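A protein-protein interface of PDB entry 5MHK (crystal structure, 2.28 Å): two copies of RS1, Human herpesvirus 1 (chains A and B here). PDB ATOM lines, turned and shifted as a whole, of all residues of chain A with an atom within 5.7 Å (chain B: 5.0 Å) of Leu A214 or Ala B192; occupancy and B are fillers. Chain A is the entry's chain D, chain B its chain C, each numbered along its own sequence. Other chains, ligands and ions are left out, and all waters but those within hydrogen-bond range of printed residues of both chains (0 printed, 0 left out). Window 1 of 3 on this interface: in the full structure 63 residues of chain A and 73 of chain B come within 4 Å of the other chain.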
ATOM      1  N   TYR A 125      18.273  17.440  19.805  1.00  0.00           N
ATOM      2  CA  TYR A 125      18.634  18.523  20.710  1.00  0.00           C
ATOM      3  C   TYR A 125      17.564  18.773  21.763  1.00  0.00           C
ATOM      4  O   TYR A 125      17.683  19.726  22.541  1.00  0.00           O
ATOM      5  CB  TYR A 125      18.908  19.806  19.923  1.00  0.00           C
ATOM      6  CG  TYR A 125      20.261  19.844  19.245  1.00  0.00           C
ATOM      7  CD1 TYR A 125      20.453  19.259  17.999  1.00  0.00           C
ATOM      8  CD2 TYR A 125      21.343  20.473  19.848  1.00  0.00           C
ATOM      9  CE1 TYR A 125      21.688  19.294  17.375  1.00  0.00           C
ATOM     10  CE2 TYR A 125      22.582  20.513  19.233  1.00  0.00           C
ATOM     11  CZ  TYR A 125      22.748  19.923  17.997  1.00  0.00           C
ATOM     12  OH  TYR A 125      23.978  19.961  17.381  1.00  0.00           O
ATOM     13  N   LEU A 189      24.568  14.487  10.936  1.00  0.00           N
ATOM     14  CA  LEU A 189      24.365  14.277  12.366  1.00  0.00           C
ATOM     15  C   LEU A 189      23.324  13.193  12.625  1.00  0.00           C
ATOM     16  O   LEU A 189      23.501  12.356  13.517  1.00  0.00           O
ATOM     17  CB  LEU A 189      23.950  15.587  13.033  1.00  0.00           C
ATOM     18  CG  LEU A 189      23.421  15.490  14.465  1.00  0.00           C
ATOM     19  CD1 LEU A 189      24.492  14.943  15.399  1.00  0.00           C
ATOM     20  CD2 LEU A 189      22.929  16.845  14.948  1.00  0.00           C
ATOM     21  N   ALA A 192      25.140   9.891  11.934  1.00  0.00           N
ATOM     22  CA  ALA A 192      26.199   9.591  12.893  1.00  0.00           C
ATOM     23  C   ALA A 192      25.628   9.233  14.260  1.00  0.00           C
ATOM     24  O   ALA A 192      26.095   8.285  14.904  1.00  0.00           O
ATOM     25  CB  ALA A 192      27.158  10.777  13.006  1.00  0.00           C
ATOM     26  N   ALA A 193      24.623   9.980  14.721  1.00  0.00           N
ATOM     27  CA  ALA A 193      23.991   9.665  15.997  1.00  0.00           C
ATOM     28  C   ALA A 193      23.263   8.328  15.942  1.00  0.00           C
ATOM     29  O   ALA A 193      23.257   7.577  16.924  1.00  0.00           O
ATOM     30  CB  ALA A 193      23.027  10.782  16.398  1.00  0.00           C
ATOM     31  N   ALA A 195      24.016   5.720  14.009  1.00  0.00           N
ATOM     32  CA  ALA A 195      24.994   4.634  13.988  1.00  0.00           C
ATOM     33  C   ALA A 195      25.496   4.325  15.392  1.00  0.00           C
ATOM     34  O   ALA A 195      25.721   3.160  15.738  1.00  0.00           O
ATOM     35  CB  ALA A 195      26.159   4.991  13.065  1.00  0.00           C
ATOM     36  N   VAL A 196      25.680   5.359  16.213  1.00  0.00           N
ATOM     37  CA  VAL A 196      26.045   5.153  17.611  1.00  0.00           C
ATOM     38  C   VAL A 196      24.907   4.476  18.364  1.00  0.00           C
ATOM     39  O   VAL A 196      25.129   3.544  19.147  1.00  0.00           O
ATOM     40  CB  VAL A 196      26.437   6.493  18.258  1.00  0.00           C
ATOM     41  CG1 VAL A 196      26.607   6.329  19.760  1.00  0.00           C
ATOM     42  CG2 VAL A 196      27.711   7.036  17.625  1.00  0.00           C
ATOM     43  N   PHE A 209      26.908  10.396  26.462  1.00  0.00           N
ATOM     44  CA  PHE A 209      28.091  11.236  26.300  1.00  0.00           C
ATOM     45  C   PHE A 209      28.369  11.517  24.830  1.00  0.00           C
ATOM     46  O   PHE A 209      28.717  12.646  24.462  1.00  0.00           O
ATOM     47  CB  PHE A 209      29.305  10.573  26.953  1.00  0.00           C
ATOM     48  CG  PHE A 209      30.608  11.277  26.674  1.00  0.00           C
ATOM     49  CD1 PHE A 209      31.023  12.334  27.467  1.00  0.00           C
ATOM     50  CD2 PHE A 209      31.422  10.874  25.624  1.00  0.00           C
ATOM     51  CE1 PHE A 209      32.221  12.983  27.216  1.00  0.00           C
ATOM     52  CE2 PHE A 209      32.619  11.518  25.367  1.00  0.00           C
ATOM     53  CZ  PHE A 209      33.020  12.574  26.164  1.00  0.00           C
ATOM     54  N   LEU A 210      28.233  10.499  23.977  1.00  0.00           N
ATOM     55  CA  LEU A 210      28.482  10.686  22.553  1.00  0.00           C
ATOM     56  C   LEU A 210      27.460  11.618  21.915  1.00  0.00           C
ATOM     57  O   LEU A 210      27.801  12.367  20.994  1.00  0.00           O
ATOM     58  CB  LEU A 210      28.499   9.333  21.843  1.00  0.00           C
ATOM     59  CG  LEU A 210      29.735   8.490  22.165  1.00  0.00           C
ATOM     60  CD1 LEU A 210      29.647   7.103  21.548  1.00  0.00           C
ATOM     61  CD2 LEU A 210      30.996   9.209  21.702  1.00  0.00           C
ATOM     62  N   LEU A 211      26.210  11.589  22.384  1.00  0.00           N
ATOM     63  CA  LEU A 211      25.218  12.528  21.870  1.00  0.00           C
ATOM     64  C   LEU A 211      25.589  13.963  22.220  1.00  0.00           C
ATOM     65  O   LEU A 211      25.459  14.867  21.386  1.00  0.00           O
ATOM     66  CB  LEU A 211      23.830  12.187  22.413  1.00  0.00           C
ATOM     67  CG  LEU A 211      22.720  13.136  21.955  1.00  0.00           C
ATOM     68  CD1 LEU A 211      22.643  13.171  20.433  1.00  0.00           C
ATOM     69  CD2 LEU A 211      21.378  12.746  22.555  1.00  0.00           C
ATOM     70  N   THR A 212      26.062  14.192  23.449  1.00  0.00           N
ATOM     71  CA  THR A 212      26.499  15.530  23.832  1.00  0.00           C
ATOM     72  C   THR A 212      27.708  15.965  23.014  1.00  0.00           C
ATOM     73  O   THR A 212      27.811  17.131  22.614  1.00  0.00           O
ATOM     74  CB  THR A 212      26.810  15.571  25.330  1.00  0.00           C
ATOM     75  OG1 THR A 212      25.592  15.423  26.072  1.00  0.00           O
ATOM     76  CG2 THR A 212      27.477  16.887  25.717  1.00  0.00           C
ATOM     77  N   SER A 213      28.627  15.037  22.740  1.00  0.00           N
ATOM     78  CA  SER A 213      29.763  15.349  21.879  1.00  0.00           C
ATOM     79  C   SER A 213      29.296  15.764  20.488  1.00  0.00           C
ATOM     80  O   SER A 213      29.765  16.766  19.936  1.00  0.00           O
ATOM     81  CB  SER A 213      30.703  14.145  21.799  1.00  0.00           C
ATOM     82  OG  SER A 213      31.789  14.402  20.927  1.00  0.00           O
ATOM     83  N   LEU A 214      28.363  15.005  19.908  1.00  0.00           N
ATOM     84  CA  LEU A 214      27.865  15.338  18.577  1.00  0.00           C
ATOM     85  C   LEU A 214      27.039  16.619  18.588  1.00  0.00           C
ATOM     86  O   LEU A 214      27.060  17.371  17.607  1.00  0.00           O
ATOM     87  CB  LEU A 214      27.043  14.176  18.018  1.00  0.00           C
ATOM     88  CG  LEU A 214      27.830  12.902  17.699  1.00  0.00           C
ATOM     89  CD1 LEU A 214      26.891  11.723  17.500  1.00  0.00           C
ATOM     90  CD2 LEU A 214      28.708  13.106  16.473  1.00  0.00           C
ATOM     91  N   ARG A 215      26.303  16.877  19.674  1.00  0.00           N
ATOM     92  CA  ARG A 215      25.557  18.127  19.788  1.00  0.00           C
ATOM     93  C   ARG A 215      26.486  19.332  19.722  1.00  0.00           C
ATOM     94  O   ARG A 215      26.232  20.286  18.980  1.00  0.00           O
ATOM     95  CB  ARG A 215      24.756  18.153  21.091  1.00  0.00           C
ATOM     96  CG  ARG A 215      23.494  17.313  21.100  1.00  0.00           C
ATOM     97  CD  ARG A 215      22.951  17.206  22.518  1.00  0.00           C
ATOM     98  NE  ARG A 215      21.631  16.587  22.571  1.00  0.00           N
ATOM     99  CZ  ARG A 215      20.999  16.282  23.700  1.00  0.00           C
ATOM    100  NH1 ARG A 215      21.569  16.536  24.870  1.00  0.00           N
ATOM    101  NH2 ARG A 215      19.797  15.722  23.661  1.00  0.00           N
ATOM    102  N   ARG A 216      27.575  19.303  20.496  1.00  0.00           N
ATOM    103  CA  ARG A 216      28.503  20.429  20.513  1.00  0.00           C
ATOM    104  C   ARG A 216      29.174  20.621  19.160  1.00  0.00           C
ATOM    105  O   ARG A 216      29.365  21.757  18.711  1.00  0.00           O
ATOM    106  CB  ARG A 216      29.552  20.237  21.607  1.00  0.00           C
ATOM    107  CG  ARG A 216      29.010  20.405  23.011  1.00  0.00           C
ATOM    108  CD  ARG A 216      30.096  20.196  24.045  1.00  0.00           C
ATOM    109  NE  ARG A 216      29.689  20.696  25.355  1.00  0.00           N
ATOM    110  CZ  ARG A 216      30.533  21.170  26.264  1.00  0.00           C
ATOM    111  NH1 ARG A 216      31.833  21.204  26.009  1.00  0.00           N
ATOM    112  NH2 ARG A 216      30.077  21.608  27.429  1.00  0.00           N
ATOM    113  N   ALA A 217      29.545  19.524  18.499  1.00  0.00           N
ATOM    114  CA  ALA A 217      30.249  19.636  17.226  1.00  0.00           C
ATOM    115  C   ALA A 217      29.346  20.217  16.145  1.00  0.00           C
ATOM    116  O   ALA A 217      29.770  21.088  15.376  1.00  0.00           O
ATOM    117  CB  ALA A 217      30.786  18.269  16.802  1.00  0.00           C
ATOM    118  N   TYR A 218      28.098  19.758  16.076  1.00  0.00           N
ATOM    119  CA  TYR A 218      27.211  20.103  14.976  1.00  0.00           C
ATOM    120  C   TYR A 218      26.405  21.373  15.216  1.00  0.00           C
ATOM    121  O   TYR A 218      25.827  21.903  14.263  1.00  0.00           O
ATOM    122  CB  TYR A 218      26.258  18.938  14.689  1.00  0.00           C
ATOM    123  CG  TYR A 218      26.864  17.884  13.790  1.00  0.00           C
ATOM    124  CD1 TYR A 218      26.745  17.970  12.410  1.00  0.00           C
ATOM    125  CD2 TYR A 218      27.566  16.810  14.324  1.00  0.00           C
ATOM    126  CE1 TYR A 218      27.302  17.012  11.585  1.00  0.00           C
ATOM    127  CE2 TYR A 218      28.126  15.846  13.507  1.00  0.00           C
ATOM    128  CZ  TYR A 218      27.990  15.953  12.138  1.00  0.00           C
ATOM    129  OH  TYR A 218      28.547  14.999  11.319  1.00  0.00           O
ATOM    130  N   ALA A 219      26.342  21.866  16.454  1.00  0.00           N
ATOM    131  CA  ALA A 219      25.536  23.054  16.733  1.00  0.00           C
ATOM    132  C   ALA A 219      25.987  24.273  15.936  1.00  0.00           C
ATOM    133  O   ALA A 219      25.128  24.919  15.308  1.00  0.00           O
ATOM    134  CB  ALA A 219      25.521  23.331  18.241  1.00  0.00           C
ATOM    135  N   GLY B 188      35.195  12.205  21.206  1.00  0.00           N
ATOM    136  CA  GLY B 188      34.012  11.528  20.705  1.00  0.00           C
ATOM    137  C   GLY B 188      34.014  11.315  19.205  1.00  0.00           C
ATOM    138  O   GLY B 188      33.302  10.433  18.715  1.00  0.00           O
ATOM    139  N   LEU B 189      34.791  12.114  18.466  1.00  0.00           N
ATOM    140  CA  LEU B 189      34.869  11.951  17.018  1.00  0.00           C
ATOM    141  C   LEU B 189      35.392  10.571  16.639  1.00  0.00           C
ATOM    142  O   LEU B 189      34.883   9.942  15.704  1.00  0.00           O
ATOM    143  CB  LEU B 189      35.753  13.041  16.411  1.00  0.00           C
ATOM    144  CG  LEU B 189      36.165  12.835  14.949  1.00  0.00           C
ATOM    145  CD1 LEU B 189      34.945  12.816  14.044  1.00  0.00           C
ATOM    146  CD2 LEU B 189      37.152  13.903  14.502  1.00  0.00           C
ATOM    147  N   ALA B 190      36.415  10.088  17.349  1.00  0.00           N
ATOM    148  CA  ALA B 190      36.968   8.771  17.050  1.00  0.00           C
ATOM    149  C   ALA B 190      35.907   7.685  17.174  1.00  0.00           C
ATOM    150  O   ALA B 190      35.879   6.741  16.377  1.00  0.00           O
ATOM    151  CB  ALA B 190      38.151   8.475  17.970  1.00  0.00           C
ATOM    152  N   HIS B 191      35.021   7.805  18.163  1.00  0.00           N
ATOM    153  CA  HIS B 191      33.982   6.800  18.360  1.00  0.00           C
ATOM    154  C   HIS B 191      32.854   6.951  17.347  1.00  0.00           C
ATOM    155  O   HIS B 191      32.342   5.950  16.832  1.00  0.00           O
ATOM    156  CB  HIS B 191      33.440   6.880  19.788  1.00  0.00           C
ATOM    157  CG  HIS B 191      34.428   6.455  20.830  1.00  0.00           C
ATOM    158  ND1 HIS B 191      34.470   5.174  21.336  1.00  0.00           N
ATOM    159  CD2 HIS B 191      35.419   7.138  21.449  1.00  0.00           C
ATOM    160  CE1 HIS B 191      35.440   5.087  22.229  1.00  0.00           C
ATOM    161  NE2 HIS B 191      36.032   6.266  22.317  1.00  0.00           N
ATOM    162  N   ALA B 192      32.449   8.189  17.051  1.00  0.00           N
ATOM    163  CA  ALA B 192      31.389   8.404  16.070  1.00  0.00           C
ATOM    164  C   ALA B 192      31.828   7.964  14.678  1.00  0.00           C
ATOM    165  O   ALA B 192      31.056   7.328  13.952  1.00  0.00           O
ATOM    166  CB  ALA B 192      30.967   9.872  16.061  1.00  0.00           C
ATOM    167  N   ALA B 193      33.061   8.295  14.288  1.00  0.00           N
ATOM    168  CA  ALA B 193      33.565   7.857  12.990  1.00  0.00           C
ATOM    169  C   ALA B 193      33.701   6.341  12.936  1.00  0.00           C
ATOM    170  O   ALA B 193      33.428   5.724  11.899  1.00  0.00           O
ATOM    171  CB  ALA B 193      34.901   8.531  12.689  1.00  0.00           C
ATOM    172  N   ALA B 194      34.116   5.723  14.044  1.00  0.00           N
ATOM    173  CA  ALA B 194      34.272   4.272  14.063  1.00  0.00           C
ATOM    174  C   ALA B 194      32.920   3.573  14.032  1.00  0.00           C
ATOM    175  O   ALA B 194      32.783   2.505  13.424  1.00  0.00           O
ATOM    176  CB  ALA B 194      35.071   3.843  15.294  1.00  0.00           C
ATOM    177  N   ALA B 195      31.910   4.156  14.683  1.00  0.00           N
ATOM    178  CA  ALA B 195      30.574   3.570  14.640  1.00  0.00           C
ATOM    179  C   ALA B 195      30.015   3.590  13.223  1.00  0.00           C
ATOM    180  O   ALA B 195      29.346   2.640  12.798  1.00  0.00           O
ATOM    181  CB  ALA B 195      29.641   4.313  15.596  1.00  0.00           C
ATOM    182  N   VAL B 196      30.272   4.667  12.480  1.00  0.00           N
ATOM    183  CA  VAL B 196      29.878   4.713  11.077  1.00  0.00           C
ATOM    184  C   VAL B 196      30.698   3.720  10.264  1.00  0.00           C
ATOM    185  O   VAL B 196      30.160   2.977   9.433  1.00  0.00           O
ATOM    186  CB  VAL B 196      30.020   6.144  10.528  1.00  0.00           C
ATOM    187  CG1 VAL B 196      29.807   6.155   9.024  1.00  0.00           C
ATOM    188  CG2 VAL B 196      29.041   7.080  11.222  1.00  0.00           C
ATOM    189  N   LEU B 214      31.738  14.858   9.557  1.00  0.00           N
ATOM    190  CA  LEU B 214      32.325  14.851  10.893  1.00  0.00           C
ATOM    191  C   LEU B 214      33.571  15.724  10.968  1.00  0.00           C
ATOM    192  O   LEU B 214      33.839  16.327  12.014  1.00  0.00           O
ATOM    193  CB  LEU B 214      32.651  13.418  11.312  1.00  0.00           C
ATOM    194  CG  LEU B 214      31.446  12.503  11.539  1.00  0.00           C
ATOM    195  CD1 LEU B 214      31.881  11.047  11.597  1.00  0.00           C
ATOM    196  CD2 LEU B 214      30.702  12.898  12.807  1.00  0.00           C
ATOM    197  N   TYR B 218      33.681  18.702  13.805  1.00  0.00           N
ATOM    198  CA  TYR B 218      34.593  18.570  14.934  1.00  0.00           C
ATOM    199  C   TYR B 218      35.834  19.444  14.833  1.00  0.00           C
ATOM    200  O   TYR B 218      36.525  19.623  15.843  1.00  0.00           O
ATOM    201  CB  TYR B 218      35.021  17.107  15.100  1.00  0.00           C
ATOM    202  CG  TYR B 218      34.046  16.279  15.906  1.00  0.00           C
ATOM    203  CD1 TYR B 218      34.165  16.187  17.288  1.00  0.00           C
ATOM    204  CD2 TYR B 218      33.005  15.597  15.290  1.00  0.00           C
ATOM    205  CE1 TYR B 218      33.277  15.436  18.033  1.00  0.00           C
ATOM    206  CE2 TYR B 218      32.110  14.843  16.029  1.00  0.00           C
ATOM    207  CZ  TYR B 218      32.252  14.766  17.400  1.00  0.00           C
ATOM    208  OH  TYR B 218      31.366  14.019  18.141  1.00  0.00           O
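The side-chain hydroxyl (OG) of Ser A213 lies within hydrogen-bond range of the side-chain hydroxyl (OH) of Tyr B218, at 2.8 Å.
Ala A195 touches Ala B195 (CB to O, 3.97 Å).
Val A196 touches Ala B195.
CA of Gly B188 touches CD2 of Leu A210, 3.9 Å away.
CD2 of Leu A210 touches CB of His B191 (3.9 Å).
Ser A213 touches Gly B188.
CD2 of Leu A214 touches CB of Ala B192, 3.97 Å away.
Leu A214 touches Tyr B218 (CD2 to OH, 3.3 Å).
CE2 of Tyr B218 touches CB of Ala A217, 3.8 Å away.
OH of Tyr A218 touches CD2 of Leu B214, 3.4 Å away.
Ala A195 touches its own counterpart, Ala B195.
Val A196 touches Ala B195, but with the chains exchanged Ala A195 does not touch Val B196 (4.01 Å).
Leu A214 touches Ala B192, but with the chains exchanged Ala A192 does not touch Leu B214 (4.1 Å).
Leu A214 touches Tyr B218, and with the chains exchanged Tyr A218 touches Leu B214.
Of the 10 pairs that touch across the chains among the printed residues, 3 have their exchanged pair printed and touching as well.
Ala B192 touches one residue of chain A.
Of the printed residues of chain B, Ala A195 touches Ala B195 (3.97 Å).
Of the printed residues of chain B, Val A196 touches Ala B195.
Phe A209 touches none of the printed residues of chain B.
Ala A192 touches none of the printed residues of chain B.
The nearest residue of chain B that does not touch Leu A214 is Leu B214 (4.2 Å).
The nearest residue of chain A that does not touch Ala B192 is Val A196 (4.2 Å).
Of the 17 printed residues of chain A, 7 touch a printed residue of chain B.
Hydrophobic or aromatic side chains of chain B within 4 Å of the printed part of chain A: His B191, Ala B192, Ala B195, Leu B214 and Tyr B218.
Among the printed residues, no Asp or Glu carboxylate lies within 4 Å of a Lys or Arg side-chain nitrogen of the other chain.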
